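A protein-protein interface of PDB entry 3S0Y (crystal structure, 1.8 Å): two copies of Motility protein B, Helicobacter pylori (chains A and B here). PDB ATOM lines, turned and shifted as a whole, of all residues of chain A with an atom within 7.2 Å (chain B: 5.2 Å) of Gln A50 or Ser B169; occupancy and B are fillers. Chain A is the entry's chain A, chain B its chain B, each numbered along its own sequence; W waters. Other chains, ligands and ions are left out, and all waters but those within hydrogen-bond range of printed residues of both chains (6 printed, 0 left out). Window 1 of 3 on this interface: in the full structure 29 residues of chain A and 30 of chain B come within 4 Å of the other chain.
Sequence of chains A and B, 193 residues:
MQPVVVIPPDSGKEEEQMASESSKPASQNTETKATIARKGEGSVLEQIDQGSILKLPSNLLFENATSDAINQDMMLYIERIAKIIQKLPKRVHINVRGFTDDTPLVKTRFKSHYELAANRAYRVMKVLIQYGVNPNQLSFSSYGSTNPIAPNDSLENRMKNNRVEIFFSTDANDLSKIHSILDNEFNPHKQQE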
ATOM      1  N   GLN A  47     -14.546  16.447  -9.396  1.00  0.00           N
ATOM      2  CA  GLN A  47     -14.453  17.883  -9.088  1.00  0.00           C
ATOM      3  C   GLN A  47     -13.018  18.324  -9.242  1.00  0.00           C
ATOM      4  O   GLN A  47     -12.115  17.692  -8.695  1.00  0.00           O
ATOM      5  CB  GLN A  47     -14.894  18.216  -7.655  1.00  0.00           C
ATOM      6  CG  GLN A  47     -15.010  19.756  -7.398  1.00  0.00           C
ATOM      7  CD  GLN A  47     -15.633  20.132  -6.066  1.00  0.00           C
ATOM      8  OE1 GLN A  47     -15.498  19.425  -5.082  1.00  0.00           O
ATOM      9  NE2 GLN A  47     -16.297  21.294  -6.034  1.00  0.00           N
ATOM     10  N   ILE A  48     -12.820  19.411  -9.988  1.00  0.00           N
ATOM     11  CA  ILE A  48     -11.543  20.112 -10.000  1.00  0.00           C
ATOM     12  C   ILE A  48     -11.818  21.533  -9.528  1.00  0.00           C
ATOM     13  O   ILE A  48     -12.966  21.899  -9.274  1.00  0.00           O
ATOM     14  CB  ILE A  48     -10.810  20.033 -11.367  1.00  0.00           C
ATOM     15  CG1 ILE A  48     -11.600  20.722 -12.493  1.00  0.00           C
ATOM     16  CG2 ILE A  48     -10.507  18.566 -11.723  1.00  0.00           C
ATOM     17  CD1 ILE A  48     -10.864  20.715 -13.835  1.00  0.00           C
ATOM     18  N   ASP A  49     -10.777  22.318  -9.315  1.00  0.00           N
ATOM     19  CA  ASP A  49     -10.984  23.574  -8.634  1.00  0.00           C
ATOM     20  C   ASP A  49     -11.662  24.610  -9.518  1.00  0.00           C
ATOM     21  O   ASP A  49     -12.232  25.564  -8.991  1.00  0.00           O
ATOM     22  CB  ASP A  49      -9.680  24.089  -8.035  1.00  0.00           C
ATOM     23  CG  ASP A  49      -9.130  23.149  -6.927  1.00  0.00           C
ATOM     24  OD1 ASP A  49      -9.801  22.158  -6.534  1.00  0.00           O
ATOM     25  OD2 ASP A  49      -8.022  23.414  -6.456  1.00  0.00           O
ATOM     26  N   GLN A  50     -11.620  24.415 -10.843  1.00  0.00           N
ATOM     27  CA  GLN A  50     -12.269  25.342 -11.794  1.00  0.00           C
ATOM     28  C   GLN A  50     -13.630  24.845 -12.309  1.00  0.00           C
ATOM     29  O   GLN A  50     -14.243  25.498 -13.149  1.00  0.00           O
ATOM     30  CB  GLN A  50     -11.375  25.590 -13.022  1.00  0.00           C
ATOM     31  CG  GLN A  50     -11.281  24.402 -14.005  1.00  0.00           C
ATOM     32  CD  GLN A  50     -10.332  24.645 -15.209  1.00  0.00           C
ATOM     33  OE1 GLN A  50     -10.595  25.471 -16.111  1.00  0.00           O
ATOM     34  NE2 GLN A  50      -9.246  23.895 -15.232  1.00  0.00           N
ATOM     35  N   GLY A  51     -14.073  23.680 -11.877  1.00  0.00           N
ATOM     36  CA  GLY A  51     -15.292  23.109 -12.448  1.00  0.00           C
ATOM     37  C   GLY A  51     -15.548  21.657 -12.127  1.00  0.00           C
ATOM     38  O   GLY A  51     -14.862  21.062 -11.288  1.00  0.00           O
ATOM     39  N   SER A  52     -16.594  21.113 -12.752  1.00  0.00           N
ATOM     40  CA  SER A  52     -16.990  19.729 -12.588  1.00  0.00           C
ATOM     41  C   SER A  52     -16.883  18.981 -13.912  1.00  0.00           C
ATOM     42  O   SER A  52     -17.164  19.545 -14.960  1.00  0.00           O
ATOM     43  CB  SER A  52     -18.425  19.648 -12.091  1.00  0.00           C
ATOM     44  OG  SER A  52     -18.545  20.167 -10.792  1.00  0.00           O
ATOM     45  N   ARG A  97     -16.457  17.136 -24.415  1.00  0.00           N
ATOM     46  CA  ARG A  97     -15.059  16.828 -24.842  1.00  0.00           C
ATOM     47  C   ARG A  97     -14.924  15.371 -25.302  1.00  0.00           C
ATOM     48  O   ARG A  97     -15.357  14.451 -24.627  1.00  0.00           O
ATOM     49  CB  ARG A  97     -14.072  17.040 -23.680  1.00  0.00           C
ATOM     50  CG  ARG A  97     -14.112  18.405 -23.044  1.00  0.00           C
ATOM     51  CD  ARG A  97     -13.311  18.495 -21.707  1.00  0.00           C
ATOM     52  NE  ARG A  97     -13.168  19.902 -21.408  1.00  0.00           N
ATOM     53  CZ  ARG A  97     -12.437  20.459 -20.447  1.00  0.00           C
ATOM     54  NH1 ARG A  97     -11.757  19.742 -19.602  1.00  0.00           N
ATOM     55  NH2 ARG A  97     -12.400  21.788 -20.374  1.00  0.00           N
ATOM     56  N   PHE A 167     -17.720  19.025 -19.248  1.00  0.00           N
ATOM     57  CA  PHE A 167     -17.100  19.972 -18.270  1.00  0.00           C
ATOM     58  C   PHE A 167     -18.000  21.182 -18.030  1.00  0.00           C
ATOM     59  O   PHE A 167     -18.443  21.840 -18.981  1.00  0.00           O
ATOM     60  CB  PHE A 167     -15.745  20.391 -18.767  1.00  0.00           C
ATOM     61  CG  PHE A 167     -15.064  21.424 -17.932  1.00  0.00           C
ATOM     62  CD1 PHE A 167     -14.692  21.164 -16.629  1.00  0.00           C
ATOM     63  CD2 PHE A 167     -14.737  22.644 -18.478  1.00  0.00           C
ATOM     64  CE1 PHE A 167     -14.019  22.145 -15.879  1.00  0.00           C
ATOM     65  CE2 PHE A 167     -14.061  23.602 -17.749  1.00  0.00           C
ATOM     66  CZ  PHE A 167     -13.715  23.355 -16.462  1.00  0.00           C
ATOM     67  N   PHE A 168     -18.287  21.426 -16.757  1.00  0.00           N
ATOM     68  CA  PHE A 168     -19.184  22.480 -16.298  1.00  0.00           C
ATOM     69  C   PHE A 168     -18.367  23.546 -15.591  1.00  0.00           C
ATOM     70  O   PHE A 168     -17.627  23.223 -14.669  1.00  0.00           O
ATOM     71  CB  PHE A 168     -20.156  21.941 -15.268  1.00  0.00           C
ATOM     72  CG  PHE A 168     -21.030  20.864 -15.771  1.00  0.00           C
ATOM     73  CD1 PHE A 168     -22.345  21.121 -16.104  1.00  0.00           C
ATOM     74  CD2 PHE A 168     -20.562  19.581 -15.885  1.00  0.00           C
ATOM     75  CE1 PHE A 168     -23.153  20.114 -16.562  1.00  0.00           C
ATOM     76  CE2 PHE A 168     -21.377  18.574 -16.329  1.00  0.00           C
ATOM     77  CZ  PHE A 168     -22.668  18.851 -16.679  1.00  0.00           C
ATOM     78  N   SER A 169     -18.513  24.792 -16.009  1.00  0.00           N
ATOM     79  CA  SER A 169     -17.698  25.880 -15.484  1.00  0.00           C
ATOM     80  C   SER A 169     -18.392  27.219 -15.690  1.00  0.00           C
ATOM     81  O   SER A 169     -19.509  27.283 -16.205  1.00  0.00           O
ATOM     82  CB  SER A 169     -16.307  25.895 -16.112  1.00  0.00           C
ATOM     83  OG  SER A 169     -16.321  26.255 -17.476  1.00  0.00           O
ATOM     84  N   THR A 170     -17.758  28.296 -15.246  1.00  0.00           N
ATOM     85  CA  THR A 170     -18.270  29.626 -15.578  1.00  0.00           C
ATOM     86  C   THR A 170     -17.114  30.519 -15.962  1.00  0.00           C
ATOM     87  O   THR A 170     -15.951  30.142 -15.781  1.00  0.00           O
ATOM     88  CB  THR A 170     -19.031  30.321 -14.428  1.00  0.00           C
ATOM     89  OG1 THR A 170     -18.107  30.789 -13.440  1.00  0.00           O
ATOM     90  CG2 THR A 170     -20.036  29.414 -13.779  1.00  0.00           C
ATOM     91  N   GLN B  50     -10.453  31.595 -13.816  1.00  0.00           N
ATOM     92  CA  GLN B  50      -9.887  30.272 -14.003  1.00  0.00           C
ATOM     93  C   GLN B  50      -8.890  30.160 -15.155  1.00  0.00           C
ATOM     94  O   GLN B  50      -8.471  29.058 -15.489  1.00  0.00           O
ATOM     95  CB  GLN B  50     -10.992  29.228 -14.083  1.00  0.00           C
ATOM     96  CG  GLN B  50     -11.883  29.197 -12.793  1.00  0.00           C
ATOM     97  CD  GLN B  50     -11.216  28.796 -11.459  1.00  0.00           C
ATOM     98  OE1 GLN B  50     -10.214  28.076 -11.393  1.00  0.00           O
ATOM     99  NE2 GLN B  50     -11.806  29.270 -10.371  1.00  0.00           N
ATOM    100  N   GLY B  51      -8.482  31.289 -15.731  1.00  0.00           N
ATOM    101  CA  GLY B  51      -7.384  31.288 -16.722  1.00  0.00           C
ATOM    102  C   GLY B  51      -7.235  32.529 -17.585  1.00  0.00           C
ATOM    103  O   GLY B  51      -7.748  33.585 -17.252  1.00  0.00           O
ATOM    104  N   ARG B  91       2.039  22.387 -15.893  1.00  0.00           N
ATOM    105  CA  ARG B  91       0.697  21.883 -15.698  1.00  0.00           C
ATOM    106  C   ARG B  91      -0.305  22.548 -16.677  1.00  0.00           C
ATOM    107  O   ARG B  91      -1.501  22.266 -16.623  1.00  0.00           O
ATOM    108  CB  ARG B  91       0.254  22.128 -14.250  1.00  0.00           C
ATOM    109  CG  ARG B  91       1.189  21.568 -13.188  1.00  0.00           C
ATOM    110  CD  ARG B  91       2.201  22.619 -12.703  1.00  0.00           C
ATOM    111  NE  ARG B  91       1.736  23.291 -11.498  1.00  0.00           N
ATOM    112  CZ  ARG B  91       2.064  22.946 -10.251  1.00  0.00           C
ATOM    113  NH1 ARG B  91       2.869  21.909 -10.002  1.00  0.00           N
ATOM    114  NH2 ARG B  91       1.570  23.645  -9.229  1.00  0.00           N
ATOM    115  N   VAL B  92       0.169  23.434 -17.547  1.00  0.00           N
ATOM    116  CA  VAL B  92      -0.742  24.241 -18.351  1.00  0.00           C
ATOM    117  C   VAL B  92      -1.387  23.378 -19.435  1.00  0.00           C
ATOM    118  O   VAL B  92      -0.764  22.485 -19.971  1.00  0.00           O
ATOM    119  CB  VAL B  92      -0.087  25.505 -18.946  1.00  0.00           C
ATOM    120  CG1 VAL B  92       1.034  25.150 -19.913  1.00  0.00           C
ATOM    121  CG2 VAL B  92      -1.140  26.381 -19.604  1.00  0.00           C
ATOM    122  N   HIS B  93      -2.670  23.616 -19.657  1.00  0.00           N
ATOM    123  CA  HIS B  93      -3.409  23.062 -20.796  1.00  0.00           C
ATOM    124  C   HIS B  93      -3.811  24.237 -21.672  1.00  0.00           C
ATOM    125  O   HIS B  93      -4.129  25.324 -21.170  1.00  0.00           O
ATOM    126  CB  HIS B  93      -4.623  22.279 -20.319  1.00  0.00           C
ATOM    127  CG  HIS B  93      -4.246  21.048 -19.551  1.00  0.00           C
ATOM    128  ND1 HIS B  93      -3.694  19.934 -20.160  1.00  0.00           N
ATOM    129  CD2 HIS B  93      -4.228  20.794 -18.219  1.00  0.00           C
ATOM    130  CE1 HIS B  93      -3.403  19.031 -19.239  1.00  0.00           C
ATOM    131  NE2 HIS B  93      -3.717  19.528 -18.052  1.00  0.00           N
ATOM    132  N   PHE B 167      -7.265  29.593 -24.854  1.00  0.00           N
ATOM    133  CA  PHE B 167      -7.501  29.570 -23.406  1.00  0.00           C
ATOM    134  C   PHE B 167      -6.439  28.723 -22.696  1.00  0.00           C
ATOM    135  O   PHE B 167      -6.193  27.555 -23.051  1.00  0.00           O
ATOM    136  CB  PHE B 167      -8.910  29.056 -23.128  1.00  0.00           C
ATOM    137  CG  PHE B 167      -9.256  28.980 -21.673  1.00  0.00           C
ATOM    138  CD1 PHE B 167      -9.325  30.126 -20.900  1.00  0.00           C
ATOM    139  CD2 PHE B 167      -9.490  27.766 -21.068  1.00  0.00           C
ATOM    140  CE1 PHE B 167      -9.633  30.051 -19.550  1.00  0.00           C
ATOM    141  CE2 PHE B 167      -9.809  27.710 -19.724  1.00  0.00           C
ATOM    142  CZ  PHE B 167      -9.865  28.861 -18.983  1.00  0.00           C
ATOM    143  N   PHE B 168      -5.808  29.338 -21.703  1.00  0.00           N
ATOM    144  CA  PHE B 168      -4.761  28.735 -20.903  1.00  0.00           C
ATOM    145  C   PHE B 168      -5.289  28.494 -19.497  1.00  0.00           C
ATOM    146  O   PHE B 168      -5.837  29.396 -18.871  1.00  0.00           O
ATOM    147  CB  PHE B 168      -3.553  29.654 -20.818  1.00  0.00           C
ATOM    148  CG  PHE B 168      -3.001  30.069 -22.163  1.00  0.00           C
ATOM    149  CD1 PHE B 168      -1.910  29.422 -22.703  1.00  0.00           C
ATOM    150  CD2 PHE B 168      -3.567  31.126 -22.864  1.00  0.00           C
ATOM    151  CE1 PHE B 168      -1.376  29.827 -23.941  1.00  0.00           C
ATOM    152  CE2 PHE B 168      -3.061  31.532 -24.091  1.00  0.00           C
ATOM    153  CZ  PHE B 168      -1.969  30.882 -24.637  1.00  0.00           C
ATOM    154  N   SER B 169      -5.145  27.271 -19.015  1.00  0.00           N
ATOM    155  CA  SER B 169      -5.662  26.878 -17.701  1.00  0.00           C
ATOM    156  C   SER B 169      -4.875  25.683 -17.125  1.00  0.00           C
ATOM    157  O   SER B 169      -3.901  25.251 -17.706  1.00  0.00           O
ATOM    158  CB  SER B 169      -7.138  26.514 -17.799  1.00  0.00           C
ATOM    159  OG  SER B 169      -7.315  25.327 -18.575  1.00  0.00           O
ATOM    160  N   THR B 170      -5.253  25.239 -15.933  1.00  0.00           N
ATOM    161  CA  THR B 170      -4.733  23.978 -15.359  1.00  0.00           C
ATOM    162  C   THR B 170      -5.883  23.165 -14.787  1.00  0.00           C
ATOM    163  O   THR B 170      -7.001  23.670 -14.630  1.00  0.00           O
ATOM    164  CB  THR B 170      -3.664  24.175 -14.234  1.00  0.00           C
ATOM    165  OG1 THR B 170      -4.298  24.572 -13.015  1.00  0.00           O
ATOM    166  CG2 THR B 170      -2.594  25.207 -14.629  1.00  0.00           C
ATOM    167  N   ASP B 171      -5.627  21.899 -14.479  1.00  0.00           N
ATOM    168  CA  ASP B 171      -6.644  21.089 -13.828  1.00  0.00           C
ATOM    169  C   ASP B 171      -6.375  20.890 -12.335  1.00  0.00           C
ATOM    170  O   ASP B 171      -6.618  19.812 -11.804  1.00  0.00           O
ATOM    171  CB  ASP B 171      -6.770  19.742 -14.520  1.00  0.00           C
ATOM    172  CG  ASP B 171      -7.482  19.839 -15.867  1.00  0.00           C
ATOM    173  OD1 ASP B 171      -8.066  20.897 -16.187  1.00  0.00           O
ATOM    174  OD2 ASP B 171      -7.448  18.833 -16.612  1.00  0.00           O
ATOM    175  N   ALA B 172      -5.899  21.949 -11.685  1.00  0.00           N
ATOM    176  CA  ALA B 172      -5.658  21.974 -10.244  1.00  0.00           C
ATOM    177  C   ALA B 172      -6.861  21.412  -9.493  1.00  0.00           C
ATOM    178  O   ALA B 172      -8.010  21.744  -9.813  1.00  0.00           O
ATOM    179  CB  ALA B 172      -5.382  23.398  -9.780  1.00  0.00           C
HETATM  180  O   HOH W   1      -7.834  26.619 -14.667  1.00  0.00           O
HETATM  181  O   HOH W   2     -13.414  31.948 -14.472  1.00  0.00           O
HETATM  182  O   HOH W   3     -10.341  23.830 -18.343  1.00  0.00           O
HETATM  183  O   HOH W   4      -8.957  23.527 -11.910  1.00  0.00           O
HETATM  184  O   HOH W   5      -9.264  18.141 -18.094  1.00  0.00           O
HETATM  185  O   HOH W   6     -10.290  21.348 -17.704  1.00  0.00           O
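Ile A48 touches Asp B171 (CD1 to OD1, 3.7 Å). Ala B172 touches Ile A48 (O to CB, 3.6 Å). Asp A49 touches Gln B50. OE1 of Gln B50 touches CB of Gln A50, at 3.2 Å. Gln A50 touches Ser B169.
N of His B93 lies within hydrogen-bond range of O of Ser B169 (2.8 Å). The backbone NH (N) of Ala B172 sits close to the side-chain hydroxyl (OG1) of Thr B170.
Gln A50 touches its own counterpart, Gln B50. Gln A50 touches Ser B169, but with the chains exchanged Ser A169 does not touch Gln B50 (6.4 Å). Gln A50 touches Thr B170, but with the chains exchanged Thr A170 does not touch Gln B50 (5.1 Å).
Water W5 bridges the side-chain carboxylate (OD2) of Asp B171 (2.4 Å) and the guanidinium group (NH1) of Arg A97 (3.3 Å). Water W1 lies within hydrogen-bond range of O of Gln B50 (2.7 Å), O of Thr B170 (3.1 Å) and NE2 of Gln A50 (3.1 Å). Water W6 lies within hydrogen-bond range of OD1 of Asp B171 (2.7 Å) and NH1 of Arg A97 (2.9 Å). Water W3 lies within hydrogen-bond range of the side-chain amide oxygen of Gln A50 (2.8 Å) and the side-chain hydroxyl of Ser B169 (3.4 Å). Water W4 lies within hydrogen-bond range of the backbone carbonyl oxygen of Ala B172, the backbone NH of Gln A50, the backbone carbonyl oxygen of Thr B170 and the backbone NH of Asp A49. Water W2 bridges N of Gln B50 and O of Thr A170.
Of the printed residues of chain B, Ile A48 touches Asp B171 (3.7 Å) and Ala B172 (3.6 Å). Of the printed residues of chain A, Gln B50 touches Asp A49 (3.98 Å) and Gln A50 (3.2 Å). Gly B51 touches none of the printed residues of chain A. Printed residues of chain A within 4 Å of Ser B169: Gln A50 (3.99 Å). Of the printed residues of chain A, Thr B170 touches Gln A50 (2.3 Å). Printed residues of chain A within 4 Å of Ala B172: Ile A48 (3.6 Å) and Asp A49 (2.9 Å). The nearest printed residue of chain B that does not touch Gln A50 is Phe B167 (4.3 Å).
Hydrophobic or aromatic side chains of chain A within 4 Å of the printed part of chain B: Ile A48. Of the 11 printed residues of chain B, 5 touch a printed residue of chain A. Along chain B the printed residues that touch a printed residue of chain A span positions 50 to 172. Among the printed residues, 8 pairs touch across the chains.
The backbone carbonyl oxygen of Ala B172 lies within hydrogen-bond range of the backbone NH of Asp A49 (2.9 Å). NE2 of Gln A50 sits at hydrogen-bond distance from OD1 of Asp B171 (3.4 Å). The backbone carbonyl oxygen of Thr B170 lies close to the side-chain amide nitrogen of Gln A50 (2.3 Å).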
